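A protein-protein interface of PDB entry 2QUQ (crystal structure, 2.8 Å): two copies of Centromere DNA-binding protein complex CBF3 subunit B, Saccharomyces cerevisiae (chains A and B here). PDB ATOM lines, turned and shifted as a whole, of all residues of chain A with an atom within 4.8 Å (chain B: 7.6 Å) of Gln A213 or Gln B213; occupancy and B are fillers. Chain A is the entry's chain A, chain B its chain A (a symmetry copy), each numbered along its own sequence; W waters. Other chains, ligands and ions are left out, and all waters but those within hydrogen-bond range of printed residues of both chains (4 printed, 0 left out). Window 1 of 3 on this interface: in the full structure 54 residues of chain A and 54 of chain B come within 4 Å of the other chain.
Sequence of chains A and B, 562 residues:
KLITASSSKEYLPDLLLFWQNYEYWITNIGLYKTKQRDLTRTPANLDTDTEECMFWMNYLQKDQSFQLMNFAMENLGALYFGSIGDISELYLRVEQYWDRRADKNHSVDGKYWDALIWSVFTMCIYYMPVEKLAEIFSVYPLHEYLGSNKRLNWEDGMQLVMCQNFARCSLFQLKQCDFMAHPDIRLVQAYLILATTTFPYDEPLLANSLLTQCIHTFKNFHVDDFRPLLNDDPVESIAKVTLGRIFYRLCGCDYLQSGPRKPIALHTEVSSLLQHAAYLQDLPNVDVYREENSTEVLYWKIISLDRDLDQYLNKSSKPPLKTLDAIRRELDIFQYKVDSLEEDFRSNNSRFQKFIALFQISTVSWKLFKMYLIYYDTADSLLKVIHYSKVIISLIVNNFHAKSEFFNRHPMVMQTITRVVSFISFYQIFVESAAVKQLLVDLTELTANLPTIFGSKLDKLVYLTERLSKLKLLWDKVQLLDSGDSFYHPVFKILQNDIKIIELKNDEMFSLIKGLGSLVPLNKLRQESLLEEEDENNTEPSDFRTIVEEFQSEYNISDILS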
ATOM      1  N   PHE A 179     -17.366  -2.015  19.551  1.00  0.00           N
ATOM      2  CA  PHE A 179     -16.959  -0.666  19.928  1.00  0.00           C
ATOM      3  C   PHE A 179     -15.466  -0.392  19.814  1.00  0.00           C
ATOM      4  O   PHE A 179     -15.058   0.756  19.640  1.00  0.00           O
ATOM      5  CB  PHE A 179     -17.452  -0.311  21.350  1.00  0.00           C
ATOM      6  CG  PHE A 179     -16.927  -1.216  22.451  1.00  0.00           C
ATOM      7  CD1 PHE A 179     -17.560  -2.418  22.752  1.00  0.00           C
ATOM      8  CD2 PHE A 179     -15.818  -0.846  23.206  1.00  0.00           C
ATOM      9  CE1 PHE A 179     -17.098  -3.232  23.785  1.00  0.00           C
ATOM     10  CE2 PHE A 179     -15.353  -1.656  24.239  1.00  0.00           C
ATOM     11  CZ  PHE A 179     -15.996  -2.849  24.525  1.00  0.00           C
ATOM     12  N   MET A 180     -14.649  -1.432  19.915  1.00  0.00           N
ATOM     13  CA  MET A 180     -13.207  -1.263  19.794  1.00  0.00           C
ATOM     14  C   MET A 180     -12.912  -0.602  18.456  1.00  0.00           C
ATOM     15  O   MET A 180     -12.072   0.290  18.349  1.00  0.00           O
ATOM     16  CB  MET A 180     -12.525  -2.623  19.838  1.00  0.00           C
ATOM     17  CG  MET A 180     -12.640  -3.314  21.170  1.00  0.00           C
ATOM     18  SD  MET A 180     -11.353  -2.804  22.305  1.00  0.00           S
ATOM     19  CE  MET A 180     -10.538  -4.340  22.546  1.00  0.00           C
ATOM     20  N   LEU A 187     -20.733   5.154  23.918  1.00  0.00           N
ATOM     21  CA  LEU A 187     -20.098   4.145  24.759  1.00  0.00           C
ATOM     22  C   LEU A 187     -19.810   4.834  26.081  1.00  0.00           C
ATOM     23  O   LEU A 187     -20.060   4.277  27.144  1.00  0.00           O
ATOM     24  CB  LEU A 187     -18.780   3.649  24.174  1.00  0.00           C
ATOM     25  CG  LEU A 187     -18.052   2.704  25.138  1.00  0.00           C
ATOM     26  CD1 LEU A 187     -18.804   1.389  25.168  1.00  0.00           C
ATOM     27  CD2 LEU A 187     -16.608   2.475  24.704  1.00  0.00           C
ATOM     28  N   SER A 209     -11.205  -1.130  32.386  1.00  0.00           N
ATOM     29  CA  SER A 209     -10.848  -1.297  30.984  1.00  0.00           C
ATOM     30  C   SER A 209     -11.846  -0.565  30.108  1.00  0.00           C
ATOM     31  O   SER A 209     -11.483  -0.018  29.072  1.00  0.00           O
ATOM     32  CB  SER A 209     -10.828  -2.774  30.626  1.00  0.00           C
ATOM     33  OG  SER A 209      -9.890  -3.455  31.438  1.00  0.00           O
ATOM     34  N   LEU A 210     -13.105  -0.558  30.531  1.00  0.00           N
ATOM     35  CA  LEU A 210     -14.147   0.128  29.793  1.00  0.00           C
ATOM     36  C   LEU A 210     -13.988   1.635  29.971  1.00  0.00           C
ATOM     37  O   LEU A 210     -14.396   2.417  29.114  1.00  0.00           O
ATOM     38  CB  LEU A 210     -15.516  -0.304  30.298  1.00  0.00           C
ATOM     39  CG  LEU A 210     -15.902  -1.752  30.021  1.00  0.00           C
ATOM     40  CD1 LEU A 210     -17.162  -2.093  30.787  1.00  0.00           C
ATOM     41  CD2 LEU A 210     -16.104  -1.937  28.529  1.00  0.00           C
ATOM     42  N   LEU A 211     -13.402   2.043  31.092  1.00  0.00           N
ATOM     43  CA  LEU A 211     -13.186   3.453  31.349  1.00  0.00           C
ATOM     44  C   LEU A 211     -12.007   3.922  30.514  1.00  0.00           C
ATOM     45  O   LEU A 211     -12.019   5.024  29.975  1.00  0.00           O
ATOM     46  CB  LEU A 211     -12.891   3.677  32.824  1.00  0.00           C
ATOM     47  CG  LEU A 211     -12.690   5.142  33.212  1.00  0.00           C
ATOM     48  CD1 LEU A 211     -13.768   6.018  32.596  1.00  0.00           C
ATOM     49  CD2 LEU A 211     -12.718   5.247  34.713  1.00  0.00           C
ATOM     50  N   THR A 212     -10.980   3.084  30.421  1.00  0.00           N
ATOM     51  CA  THR A 212      -9.804   3.410  29.635  1.00  0.00           C
ATOM     52  C   THR A 212     -10.303   3.579  28.210  1.00  0.00           C
ATOM     53  O   THR A 212      -9.930   4.531  27.524  1.00  0.00           O
ATOM     54  CB  THR A 212      -8.731   2.287  29.716  1.00  0.00           C
ATOM     55  OG1 THR A 212      -8.333   2.118  31.077  1.00  0.00           O
ATOM     56  CG2 THR A 212      -7.494   2.653  28.934  1.00  0.00           C
ATOM     57  N   GLN A 213     -11.159   2.662  27.766  1.00  0.00           N
ATOM     58  CA  GLN A 213     -11.722   2.764  26.426  1.00  0.00           C
ATOM     59  C   GLN A 213     -12.473   4.090  26.278  1.00  0.00           C
ATOM     60  O   GLN A 213     -12.456   4.700  25.203  1.00  0.00           O
ATOM     61  CB  GLN A 213     -12.678   1.600  26.136  1.00  0.00           C
ATOM     62  CG  GLN A 213     -11.996   0.361  25.615  1.00  0.00           C
ATOM     63  CD  GLN A 213     -11.142   0.650  24.388  1.00  0.00           C
ATOM     64  OE1 GLN A 213     -11.651   1.096  23.336  1.00  0.00           O
ATOM     65  NE2 GLN A 213      -9.835   0.405  24.514  1.00  0.00           N
ATOM     66  N   CYS A 214     -13.126   4.532  27.356  1.00  0.00           N
ATOM     67  CA  CYS A 214     -13.879   5.781  27.340  1.00  0.00           C
ATOM     68  C   CYS A 214     -12.938   6.974  27.303  1.00  0.00           C
ATOM     69  O   CYS A 214     -13.235   7.971  26.643  1.00  0.00           O
ATOM     70  CB  CYS A 214     -14.789   5.876  28.556  1.00  0.00           C
ATOM     71  SG  CYS A 214     -16.166   4.738  28.528  1.00  0.00           S
ATOM     72  N   ILE A 215     -11.814   6.892  28.021  1.00  0.00           N
ATOM     73  CA  ILE A 215     -10.840   7.978  27.987  1.00  0.00           C
ATOM     74  C   ILE A 215     -10.402   8.079  26.525  1.00  0.00           C
ATOM     75  O   ILE A 215     -10.462   9.148  25.931  1.00  0.00           O
ATOM     76  CB  ILE A 215      -9.598   7.692  28.853  1.00  0.00           C
ATOM     77  CG1 ILE A 215     -10.015   7.362  30.289  1.00  0.00           C
ATOM     78  CG2 ILE A 215      -8.663   8.884  28.825  1.00  0.00           C
ATOM     79  CD1 ILE A 215     -10.994   8.289  30.850  1.00  0.00           C
ATOM     80  N   HIS A 216      -9.987   6.949  25.951  1.00  0.00           N
ATOM     81  CA  HIS A 216      -9.570   6.864  24.549  1.00  0.00           C
ATOM     82  C   HIS A 216     -10.636   7.457  23.595  1.00  0.00           C
ATOM     83  O   HIS A 216     -10.357   8.324  22.771  1.00  0.00           O
ATOM     84  CB  HIS A 216      -9.297   5.389  24.202  1.00  0.00           C
ATOM     85  CG  HIS A 216      -9.179   5.102  22.731  1.00  0.00           C
ATOM     86  ND1 HIS A 216      -8.301   5.771  21.902  1.00  0.00           N
ATOM     87  CD2 HIS A 216      -9.818   4.199  21.948  1.00  0.00           C
ATOM     88  CE1 HIS A 216      -8.407   5.294  20.674  1.00  0.00           C
ATOM     89  NE2 HIS A 216      -9.319   4.340  20.674  1.00  0.00           N
ATOM     90  N   THR A 217     -11.863   6.979  23.716  1.00  0.00           N
ATOM     91  CA  THR A 217     -12.938   7.461  22.870  1.00  0.00           C
ATOM     92  C   THR A 217     -13.169   8.944  23.027  1.00  0.00           C
ATOM     93  O   THR A 217     -13.498   9.626  22.063  1.00  0.00           O
ATOM     94  CB  THR A 217     -14.260   6.753  23.189  1.00  0.00           C
ATOM     95  OG1 THR A 217     -14.195   5.390  22.751  1.00  0.00           O
ATOM     96  CG2 THR A 217     -15.406   7.453  22.505  1.00  0.00           C
ATOM     97  N   PHE B 179     -10.791 -10.440  27.991  1.00  0.00           N
ATOM     98  CA  PHE B 179      -9.567  -9.748  28.381  1.00  0.00           C
ATOM     99  C   PHE B 179      -9.782  -8.421  29.097  1.00  0.00           C
ATOM    100  O   PHE B 179      -8.926  -7.986  29.866  1.00  0.00           O
ATOM    101  CB  PHE B 179      -8.630  -9.546  27.169  1.00  0.00           C
ATOM    102  CG  PHE B 179      -9.218  -8.721  26.037  1.00  0.00           C
ATOM    103  CD1 PHE B 179     -10.017  -9.312  25.063  1.00  0.00           C
ATOM    104  CD2 PHE B 179      -8.946  -7.360  25.933  1.00  0.00           C
ATOM    105  CE1 PHE B 179     -10.531  -8.561  24.006  1.00  0.00           C
ATOM    106  CE2 PHE B 179      -9.455  -6.607  24.879  1.00  0.00           C
ATOM    107  CZ  PHE B 179     -10.248  -7.212  23.917  1.00  0.00           C
ATOM    108  N   MET B 180     -10.913  -7.774  28.848  1.00  0.00           N
ATOM    109  CA  MET B 180     -11.210  -6.510  29.508  1.00  0.00           C
ATOM    110  C   MET B 180     -11.152  -6.729  31.012  1.00  0.00           C
ATOM    111  O   MET B 180     -10.624  -5.909  31.763  1.00  0.00           O
ATOM    112  CB  MET B 180     -12.609  -6.047  29.127  1.00  0.00           C
ATOM    113  CG  MET B 180     -12.747  -5.674  27.675  1.00  0.00           C
ATOM    114  SD  MET B 180     -12.271  -3.975  27.370  1.00  0.00           S
ATOM    115  CE  MET B 180     -13.799  -3.332  26.794  1.00  0.00           C
ATOM    116  N   ALA B 181     -11.688  -7.868  31.426  1.00  0.00           N
ATOM    117  CA  ALA B 181     -11.762  -8.257  32.824  1.00  0.00           C
ATOM    118  C   ALA B 181     -10.568  -9.048  33.368  1.00  0.00           C
ATOM    119  O   ALA B 181     -10.432  -9.210  34.580  1.00  0.00           O
ATOM    120  CB  ALA B 181     -13.035  -9.048  33.039  1.00  0.00           C
ATOM    121  N   PRO B 183      -6.746  -8.782  32.496  1.00  0.00           N
ATOM    122  CA  PRO B 183      -5.495  -8.375  31.852  1.00  0.00           C
ATOM    123  C   PRO B 183      -4.353  -9.373  32.025  1.00  0.00           C
ATOM    124  O   PRO B 183      -4.109  -9.873  33.126  1.00  0.00           O
ATOM    125  CB  PRO B 183      -5.203  -7.016  32.485  1.00  0.00           C
ATOM    126  CG  PRO B 183      -6.026  -7.023  33.748  1.00  0.00           C
ATOM    127  CD  PRO B 183      -7.278  -7.706  33.338  1.00  0.00           C
ATOM    128  N   ASP B 184      -3.656  -9.658  30.928  1.00  0.00           N
ATOM    129  CA  ASP B 184      -2.547 -10.605  30.949  1.00  0.00           C
ATOM    130  C   ASP B 184      -1.488 -10.103  29.957  1.00  0.00           C
ATOM    131  O   ASP B 184      -1.837  -9.388  29.026  1.00  0.00           O
ATOM    132  CB  ASP B 184      -3.086 -11.979  30.547  1.00  0.00           C
ATOM    133  CG  ASP B 184      -2.217 -13.113  31.032  1.00  0.00           C
ATOM    134  OD1 ASP B 184      -1.143 -13.335  30.438  1.00  0.00           O
ATOM    135  OD2 ASP B 184      -2.604 -13.785  32.011  1.00  0.00           O
ATOM    136  N   LEU B 187      -1.928 -10.729  26.210  1.00  0.00           N
ATOM    137  CA  LEU B 187      -2.730  -9.928  25.291  1.00  0.00           C
ATOM    138  C   LEU B 187      -1.747  -9.026  24.567  1.00  0.00           C
ATOM    139  O   LEU B 187      -1.817  -8.870  23.353  1.00  0.00           O
ATOM    140  CB  LEU B 187      -3.745  -9.053  26.018  1.00  0.00           C
ATOM    141  CG  LEU B 187      -4.475  -8.110  25.054  1.00  0.00           C
ATOM    142  CD1 LEU B 187      -5.432  -8.936  24.219  1.00  0.00           C
ATOM    143  CD2 LEU B 187      -5.235  -7.026  25.809  1.00  0.00           C
ATOM    144  N   VAL B 188      -0.828  -8.435  25.326  1.00  0.00           N
ATOM    145  CA  VAL B 188       0.181  -7.552  24.765  1.00  0.00           C
ATOM    146  C   VAL B 188       1.103  -8.343  23.840  1.00  0.00           C
ATOM    147  O   VAL B 188       1.640  -7.812  22.855  1.00  0.00           O
ATOM    148  CB  VAL B 188       1.033  -6.952  25.875  1.00  0.00           C
ATOM    149  CG1 VAL B 188       2.038  -5.959  25.311  1.00  0.00           C
ATOM    150  CG2 VAL B 188       0.136  -6.324  26.903  1.00  0.00           C
ATOM    151  N   LEU B 205      -8.655   1.434  13.462  1.00  0.00           N
ATOM    152  CA  LEU B 205      -9.448   1.801  14.616  1.00  0.00           C
ATOM    153  C   LEU B 205      -9.422   0.751  15.712  1.00  0.00           C
ATOM    154  O   LEU B 205      -9.337   1.079  16.887  1.00  0.00           O
ATOM    155  CB  LEU B 205     -10.875   2.063  14.183  1.00  0.00           C
ATOM    156  CG  LEU B 205     -10.919   3.278  13.273  1.00  0.00           C
ATOM    157  CD1 LEU B 205     -12.356   3.609  12.967  1.00  0.00           C
ATOM    158  CD2 LEU B 205     -10.230   4.445  13.960  1.00  0.00           C
ATOM    159  N   LEU B 206      -9.491  -0.513  15.321  1.00  0.00           N
ATOM    160  CA  LEU B 206      -9.482  -1.622  16.266  1.00  0.00           C
ATOM    161  C   LEU B 206      -8.122  -1.754  16.900  1.00  0.00           C
ATOM    162  O   LEU B 206      -8.002  -1.887  18.114  1.00  0.00           O
ATOM    163  CB  LEU B 206      -9.830  -2.938  15.551  1.00  0.00           C
ATOM    164  CG  LEU B 206      -9.721  -4.268  16.312  1.00  0.00           C
ATOM    165  CD1 LEU B 206     -10.857  -4.413  17.327  1.00  0.00           C
ATOM    166  CD2 LEU B 206      -9.776  -5.407  15.320  1.00  0.00           C
ATOM    167  N   ALA B 207      -7.093  -1.718  16.066  1.00  0.00           N
ATOM    168  CA  ALA B 207      -5.720  -1.859  16.524  1.00  0.00           C
ATOM    169  C   ALA B 207      -5.332  -0.767  17.519  1.00  0.00           C
ATOM    170  O   ALA B 207      -4.531  -0.992  18.431  1.00  0.00           O
ATOM    171  CB  ALA B 207      -4.793  -1.850  15.334  1.00  0.00           C
ATOM    172  N   ASN B 208      -5.899   0.420  17.349  1.00  0.00           N
ATOM    173  CA  ASN B 208      -5.608   1.501  18.274  1.00  0.00           C
ATOM    174  C   ASN B 208      -6.245   1.273  19.640  1.00  0.00           C
ATOM    175  O   ASN B 208      -5.688   1.668  20.662  1.00  0.00           O
ATOM    176  CB  ASN B 208      -6.066   2.827  17.687  1.00  0.00           C
ATOM    177  CG  ASN B 208      -5.125   3.322  16.627  1.00  0.00           C
ATOM    178  OD1 ASN B 208      -4.183   2.620  16.245  1.00  0.00           O
ATOM    179  ND2 ASN B 208      -5.360   4.532  16.143  1.00  0.00           N
ATOM    180  N   SER B 209      -7.407   0.625  19.648  1.00  0.00           N
ATOM    181  CA  SER B 209      -8.131   0.332  20.877  1.00  0.00           C
ATOM    182  C   SER B 209      -7.487  -0.844  21.586  1.00  0.00           C
ATOM    183  O   SER B 209      -7.448  -0.888  22.811  1.00  0.00           O
ATOM    184  CB  SER B 209      -9.583   0.015  20.561  1.00  0.00           C
ATOM    185  OG  SER B 209     -10.186   1.116  19.907  1.00  0.00           O
ATOM    186  N   LEU B 210      -6.982  -1.794  20.809  1.00  0.00           N
ATOM    187  CA  LEU B 210      -6.321  -2.956  21.367  1.00  0.00           C
ATOM    188  C   LEU B 210      -4.953  -2.551  21.908  1.00  0.00           C
ATOM    189  O   LEU B 210      -4.424  -3.183  22.822  1.00  0.00           O
ATOM    190  CB  LEU B 210      -6.151  -4.026  20.298  1.00  0.00           C
ATOM    191  CG  LEU B 210      -7.435  -4.669  19.789  1.00  0.00           C
ATOM    192  CD1 LEU B 210      -7.126  -5.519  18.575  1.00  0.00           C
ATOM    193  CD2 LEU B 210      -8.048  -5.503  20.898  1.00  0.00           C
ATOM    194  N   LEU B 211      -4.374  -1.502  21.335  1.00  0.00           N
ATOM    195  CA  LEU B 211      -3.081  -1.024  21.788  1.00  0.00           C
ATOM    196  C   LEU B 211      -3.276  -0.260  23.087  1.00  0.00           C
ATOM    197  O   LEU B 211      -2.465  -0.362  24.001  1.00  0.00           O
ATOM    198  CB  LEU B 211      -2.466  -0.108  20.741  1.00  0.00           C
ATOM    199  CG  LEU B 211      -1.077   0.418  21.102  1.00  0.00           C
ATOM    200  CD1 LEU B 211      -0.194  -0.702  21.627  1.00  0.00           C
ATOM    201  CD2 LEU B 211      -0.469   1.040  19.874  1.00  0.00           C
ATOM    202  N   THR B 212      -4.350   0.519  23.157  1.00  0.00           N
ATOM    203  CA  THR B 212      -4.655   1.283  24.353  1.00  0.00           C
ATOM    204  C   THR B 212      -4.844   0.254  25.454  1.00  0.00           C
ATOM    205  O   THR B 212      -4.326   0.416  26.559  1.00  0.00           O
ATOM    206  CB  THR B 212      -5.940   2.141  24.173  1.00  0.00           C
ATOM    207  OG1 THR B 212      -5.745   3.053  23.091  1.00  0.00           O
ATOM    208  CG2 THR B 212      -6.226   2.967  25.403  1.00  0.00           C
ATOM    209  N   GLN B 213      -5.574  -0.816  25.151  1.00  0.00           N
ATOM    210  CA  GLN B 213      -5.776  -1.875  26.132  1.00  0.00           C
ATOM    211  C   GLN B 213      -4.423  -2.448  26.564  1.00  0.00           C
ATOM    212  O   GLN B 213      -4.243  -2.810  27.731  1.00  0.00           O
ATOM    213  CB  GLN B 213      -6.649  -3.000  25.561  1.00  0.00           C
ATOM    214  CG  GLN B 213      -8.130  -2.762  25.707  1.00  0.00           C
ATOM    215  CD  GLN B 213      -8.526  -2.478  27.149  1.00  0.00           C
ATOM    216  OE1 GLN B 213      -8.337  -3.324  28.050  1.00  0.00           O
ATOM    217  NE2 GLN B 213      -9.073  -1.281  27.380  1.00  0.00           N
ATOM    218  N   CYS B 214      -3.477  -2.523  25.623  1.00  0.00           N
ATOM    219  CA  CYS B 214      -2.149  -3.051  25.911  1.00  0.00           C
ATOM    220  C   CYS B 214      -1.357  -2.074  26.763  1.00  0.00           C
ATOM    221  O   CYS B 214      -0.600  -2.497  27.639  1.00  0.00           O
ATOM    222  CB  CYS B 214      -1.396  -3.342  24.620  1.00  0.00           C
ATOM    223  SG  CYS B 214      -2.037  -4.732  23.698  1.00  0.00           S
ATOM    224  N   ILE B 215      -1.505  -0.772  26.503  1.00  0.00           N
ATOM    225  CA  ILE B 215      -0.817   0.223  27.320  1.00  0.00           C
ATOM    226  C   ILE B 215      -1.344   0.011  28.741  1.00  0.00           C
ATOM    227  O   ILE B 215      -0.568  -0.161  29.671  1.00  0.00           O
ATOM    228  CB  ILE B 215      -1.133   1.669  26.889  1.00  0.00           C
ATOM    229  CG1 ILE B 215      -0.826   1.859  25.402  1.00  0.00           C
ATOM    230  CG2 ILE B 215      -0.337   2.644  27.732  1.00  0.00           C
ATOM    231  CD1 ILE B 215       0.472   1.333  24.990  1.00  0.00           C
ATOM    232  N   HIS B 216      -2.670   0.001  28.886  1.00  0.00           N
ATOM    233  CA  HIS B 216      -3.337  -0.227  30.170  1.00  0.00           C
ATOM    234  C   HIS B 216      -2.825  -1.514  30.863  1.00  0.00           C
ATOM    235  O   HIS B 216      -2.404  -1.504  32.016  1.00  0.00           O
ATOM    236  CB  HIS B 216      -4.856  -0.312  29.930  1.00  0.00           C
ATOM    237  CG  HIS B 216      -5.643  -0.864  31.087  1.00  0.00           C
ATOM    238  ND1 HIS B 216      -5.571  -0.343  32.363  1.00  0.00           N
ATOM    239  CD2 HIS B 216      -6.537  -1.879  31.148  1.00  0.00           C
ATOM    240  CE1 HIS B 216      -6.383  -1.015  33.158  1.00  0.00           C
ATOM    241  NE2 HIS B 216      -6.982  -1.952  32.447  1.00  0.00           N
ATOM    242  N   THR B 217      -2.866  -2.624  30.145  1.00  0.00           N
ATOM    243  CA  THR B 217      -2.415  -3.887  30.698  1.00  0.00           C
ATOM    244  C   THR B 217      -0.966  -3.844  31.114  1.00  0.00           C
ATOM    245  O   THR B 217      -0.585  -4.462  32.103  1.00  0.00           O
ATOM    246  CB  THR B 217      -2.569  -5.027  29.684  1.00  0.00           C
ATOM    247  OG1 THR B 217      -3.959  -5.322  29.498  1.00  0.00           O
ATOM    248  CG2 THR B 217      -1.847  -6.258  30.168  1.00  0.00           C
ATOM    249  N   PHE B 218      -0.154  -3.121  30.357  1.00  0.00           N
ATOM    250  CA  PHE B 218       1.264  -3.060  30.670  1.00  0.00           C
ATOM    251  C   PHE B 218       1.569  -2.279  31.932  1.00  0.00           C
ATOM    252  O   PHE B 218       2.388  -2.689  32.754  1.00  0.00           O
ATOM    253  CB  PHE B 218       2.055  -2.436  29.531  1.00  0.00           C
ATOM    254  CG  PHE B 218       3.517  -2.327  29.836  1.00  0.00           C
ATOM    255  CD1 PHE B 218       4.341  -3.446  29.754  1.00  0.00           C
ATOM    256  CD2 PHE B 218       4.053  -1.139  30.315  1.00  0.00           C
ATOM    257  CE1 PHE B 218       5.670  -3.389  30.148  1.00  0.00           C
ATOM    258  CE2 PHE B 218       5.379  -1.067  30.715  1.00  0.00           C
ATOM    259  CZ  PHE B 218       6.189  -2.194  30.633  1.00  0.00           C
ATOM    260  N   LYS B 219       0.920  -1.135  32.071  1.00  0.00           N
ATOM    261  CA  LYS B 219       1.142  -0.292  33.222  1.00  0.00           C
ATOM    262  C   LYS B 219       0.521  -0.932  34.449  1.00  0.00           C
ATOM    263  O   LYS B 219       0.911  -0.666  35.572  1.00  0.00           O
ATOM    264  CB  LYS B 219       0.552   1.088  32.951  1.00  0.00           C
ATOM    265  CG  LYS B 219       1.182   1.764  31.730  1.00  0.00           C
ATOM    266  CD  LYS B 219       0.413   3.020  31.286  1.00  0.00           C
ATOM    267  CE  LYS B 219       0.865   4.281  32.013  1.00  0.00           C
ATOM    268  NZ  LYS B 219       2.249   4.662  31.646  1.00  0.00           N
ATOM    269  N   ASN B 220      -0.443  -1.804  34.225  1.00  0.00           N
ATOM    270  CA  ASN B 220      -1.110  -2.487  35.313  1.00  0.00           C
ATOM    271  C   ASN B 220      -0.129  -3.347  36.131  1.00  0.00           C
ATOM    272  O   ASN B 220      -0.444  -3.744  37.245  1.00  0.00           O
ATOM    273  CB  ASN B 220      -2.219  -3.344  34.724  1.00  0.00           C
ATOM    274  CG  ASN B 220      -3.141  -3.888  35.760  1.00  0.00           C
ATOM    275  OD1 ASN B 220      -3.839  -3.142  36.429  1.00  0.00           O
ATOM    276  ND2 ASN B 220      -3.159  -5.202  35.900  1.00  0.00           N
ATOM    277  N   LEU B 250       6.637  -2.682  22.519  1.00  0.00           N
ATOM    278  CA  LEU B 250       5.360  -1.994  22.631  1.00  0.00           C
ATOM    279  C   LEU B 250       5.481  -0.499  22.322  1.00  0.00           C
ATOM    280  O   LEU B 250       4.585   0.072  21.714  1.00  0.00           O
ATOM    281  CB  LEU B 250       4.786  -2.203  24.028  1.00  0.00           C
ATOM    282  CG  LEU B 250       3.362  -1.730  24.316  1.00  0.00           C
ATOM    283  CD1 LEU B 250       2.397  -2.286  23.277  1.00  0.00           C
ATOM    284  CD2 LEU B 250       2.970  -2.184  25.718  1.00  0.00           C
ATOM    285  N   ILE B 264      -3.942   8.164  23.145  1.00  0.00           N
ATOM    286  CA  ILE B 264      -3.211   7.767  24.346  1.00  0.00           C
ATOM    287  C   ILE B 264      -1.816   7.256  23.981  1.00  0.00           C
ATOM    288  O   ILE B 264      -1.672   6.427  23.092  1.00  0.00           O
ATOM    289  CB  ILE B 264      -4.033   6.706  25.111  1.00  0.00           C
ATOM    290  CG1 ILE B 264      -5.306   7.371  25.662  1.00  0.00           C
ATOM    291  CG2 ILE B 264      -3.205   6.073  26.209  1.00  0.00           C
ATOM    292  CD1 ILE B 264      -6.330   6.407  26.183  1.00  0.00           C
HETATM  293  O   HOH W   1      -6.436   2.600  32.868  1.00  0.00           O
HETATM  294  O   HOH W   2      -8.332  -3.880  33.958  1.00  0.00           O
HETATM  295  O   HOH W   3      -5.244   5.572  22.428  1.00  0.00           O
HETATM  296  O   HOH W   4     -10.158   3.527  18.134  1.00  0.00           O
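O of Met A180 is in hydrogen-bond range of OG of Ser B209. The backbone carbonyl oxygen of Met B180 sits at hydrogen-bond distance from the side-chain hydroxyl of Ser A209, at 2.6 Å. O of Ser A209 sits at hydrogen-bond distance from NE2 of Gln B213. A ring nitrogen (NE2) of His B216 is in hydrogen-bond range of the side-chain hydroxyl (OG) of Ser A209. NE2 of Gln A213 lies within hydrogen-bond range of O of Ser B209, 3.2 Å away. The side-chain amide nitrogen (NE2) of Gln B213 sits close to the side-chain amide nitrogen (NE2) of Gln A213 (3.4 Å). NE2 of His A216 is in hydrogen-bond range of OG of Ser B209 (3.4 Å). O of Leu B205 sits close to O of Met A180.
The backbone carbonyl oxygen of Gln A213 is in hydrogen-bond range of the side-chain hydroxyl of Thr A217 (3.1 Å). The side-chain hydroxyl (OG) of Ser B209 lies within hydrogen-bond range of the backbone carbonyl oxygen (O) of Leu B205, 3.1 Å away. The backbone carbonyl oxygen of Asn B208 sits at hydrogen-bond distance from the side-chain hydroxyl of Thr B212. The side-chain sulfur of Cys B214 lies within hydrogen-bond range of the backbone carbonyl oxygen of Leu B210 (3.0 Å).
CZ of Phe A179 touches CE of Met B180, 3.2 Å away. CZ of Phe B179 touches CE of Met A180, at 3.2 Å. Met A180 touches Leu B206. Met A180 touches Leu B210 (CE to CD2, 3.2 Å). Leu A210 touches Met B180. Thr A212 touches Thr B212. Thr A212 touches His B216. His A216 touches Thr B212 (ND1 to OG1, 3.9 Å). His A216 touches Ile B264.
Of chain B, only Ser B209 and Gln B213 come within 4 Å of Gln A213. Of the printed residues of chain B, His A216 touches Ser B209, Thr B212 and Ile B264. Of the printed residues of chain A, Phe B179 touches Met A180. Gln B213 touches just these residues of chain A: Ser A209 and Gln A213. Of the printed residues of chain A, Ile B264 touches His A216.
Of the 25 printed residues of chain B, 10 touch a printed residue of chain A. Hydrophobic or aromatic side chains of chain B within 4 Å of the printed part of chain A: Phe B179, Met B180, Leu B206, Leu B210, His B216 and Ile B264. Among the printed residues, no Asp or Glu carboxylate lies within 4 Å of a Lys or Arg side-chain nitrogen of the other chain.
Met A180 touches Ser B209, and with the chains exchanged Ser A209 touches Met B180. Thr A212 touches its own counterpart, Thr B212. Thr A212 touches His B216, and with the chains exchanged His A216 touches Thr B212. Gln B213 touches its own counterpart, Gln A213. Positions printed for both chains: 179, 180, 187, 209, 210, 211, 212, 213, 214, 215, 216 and 217.
Water W1 bridges the side-chain hydroxyl (OG1) of Thr A212 (2.7 Å) and a ring nitrogen (ND1) of His B216 (3.1 Å). Water W3 lies within hydrogen-bond range of the side-chain hydroxyl of Thr B212 (2.7 Å), the backbone NH of Ile B264 (3.0 Å) and a ring nitrogen (ND1) of His A216 (3.1 Å). Water W2 bridges NE2 of His B216 (2.8 Å) and OG of Ser A209 (3.0 Å).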
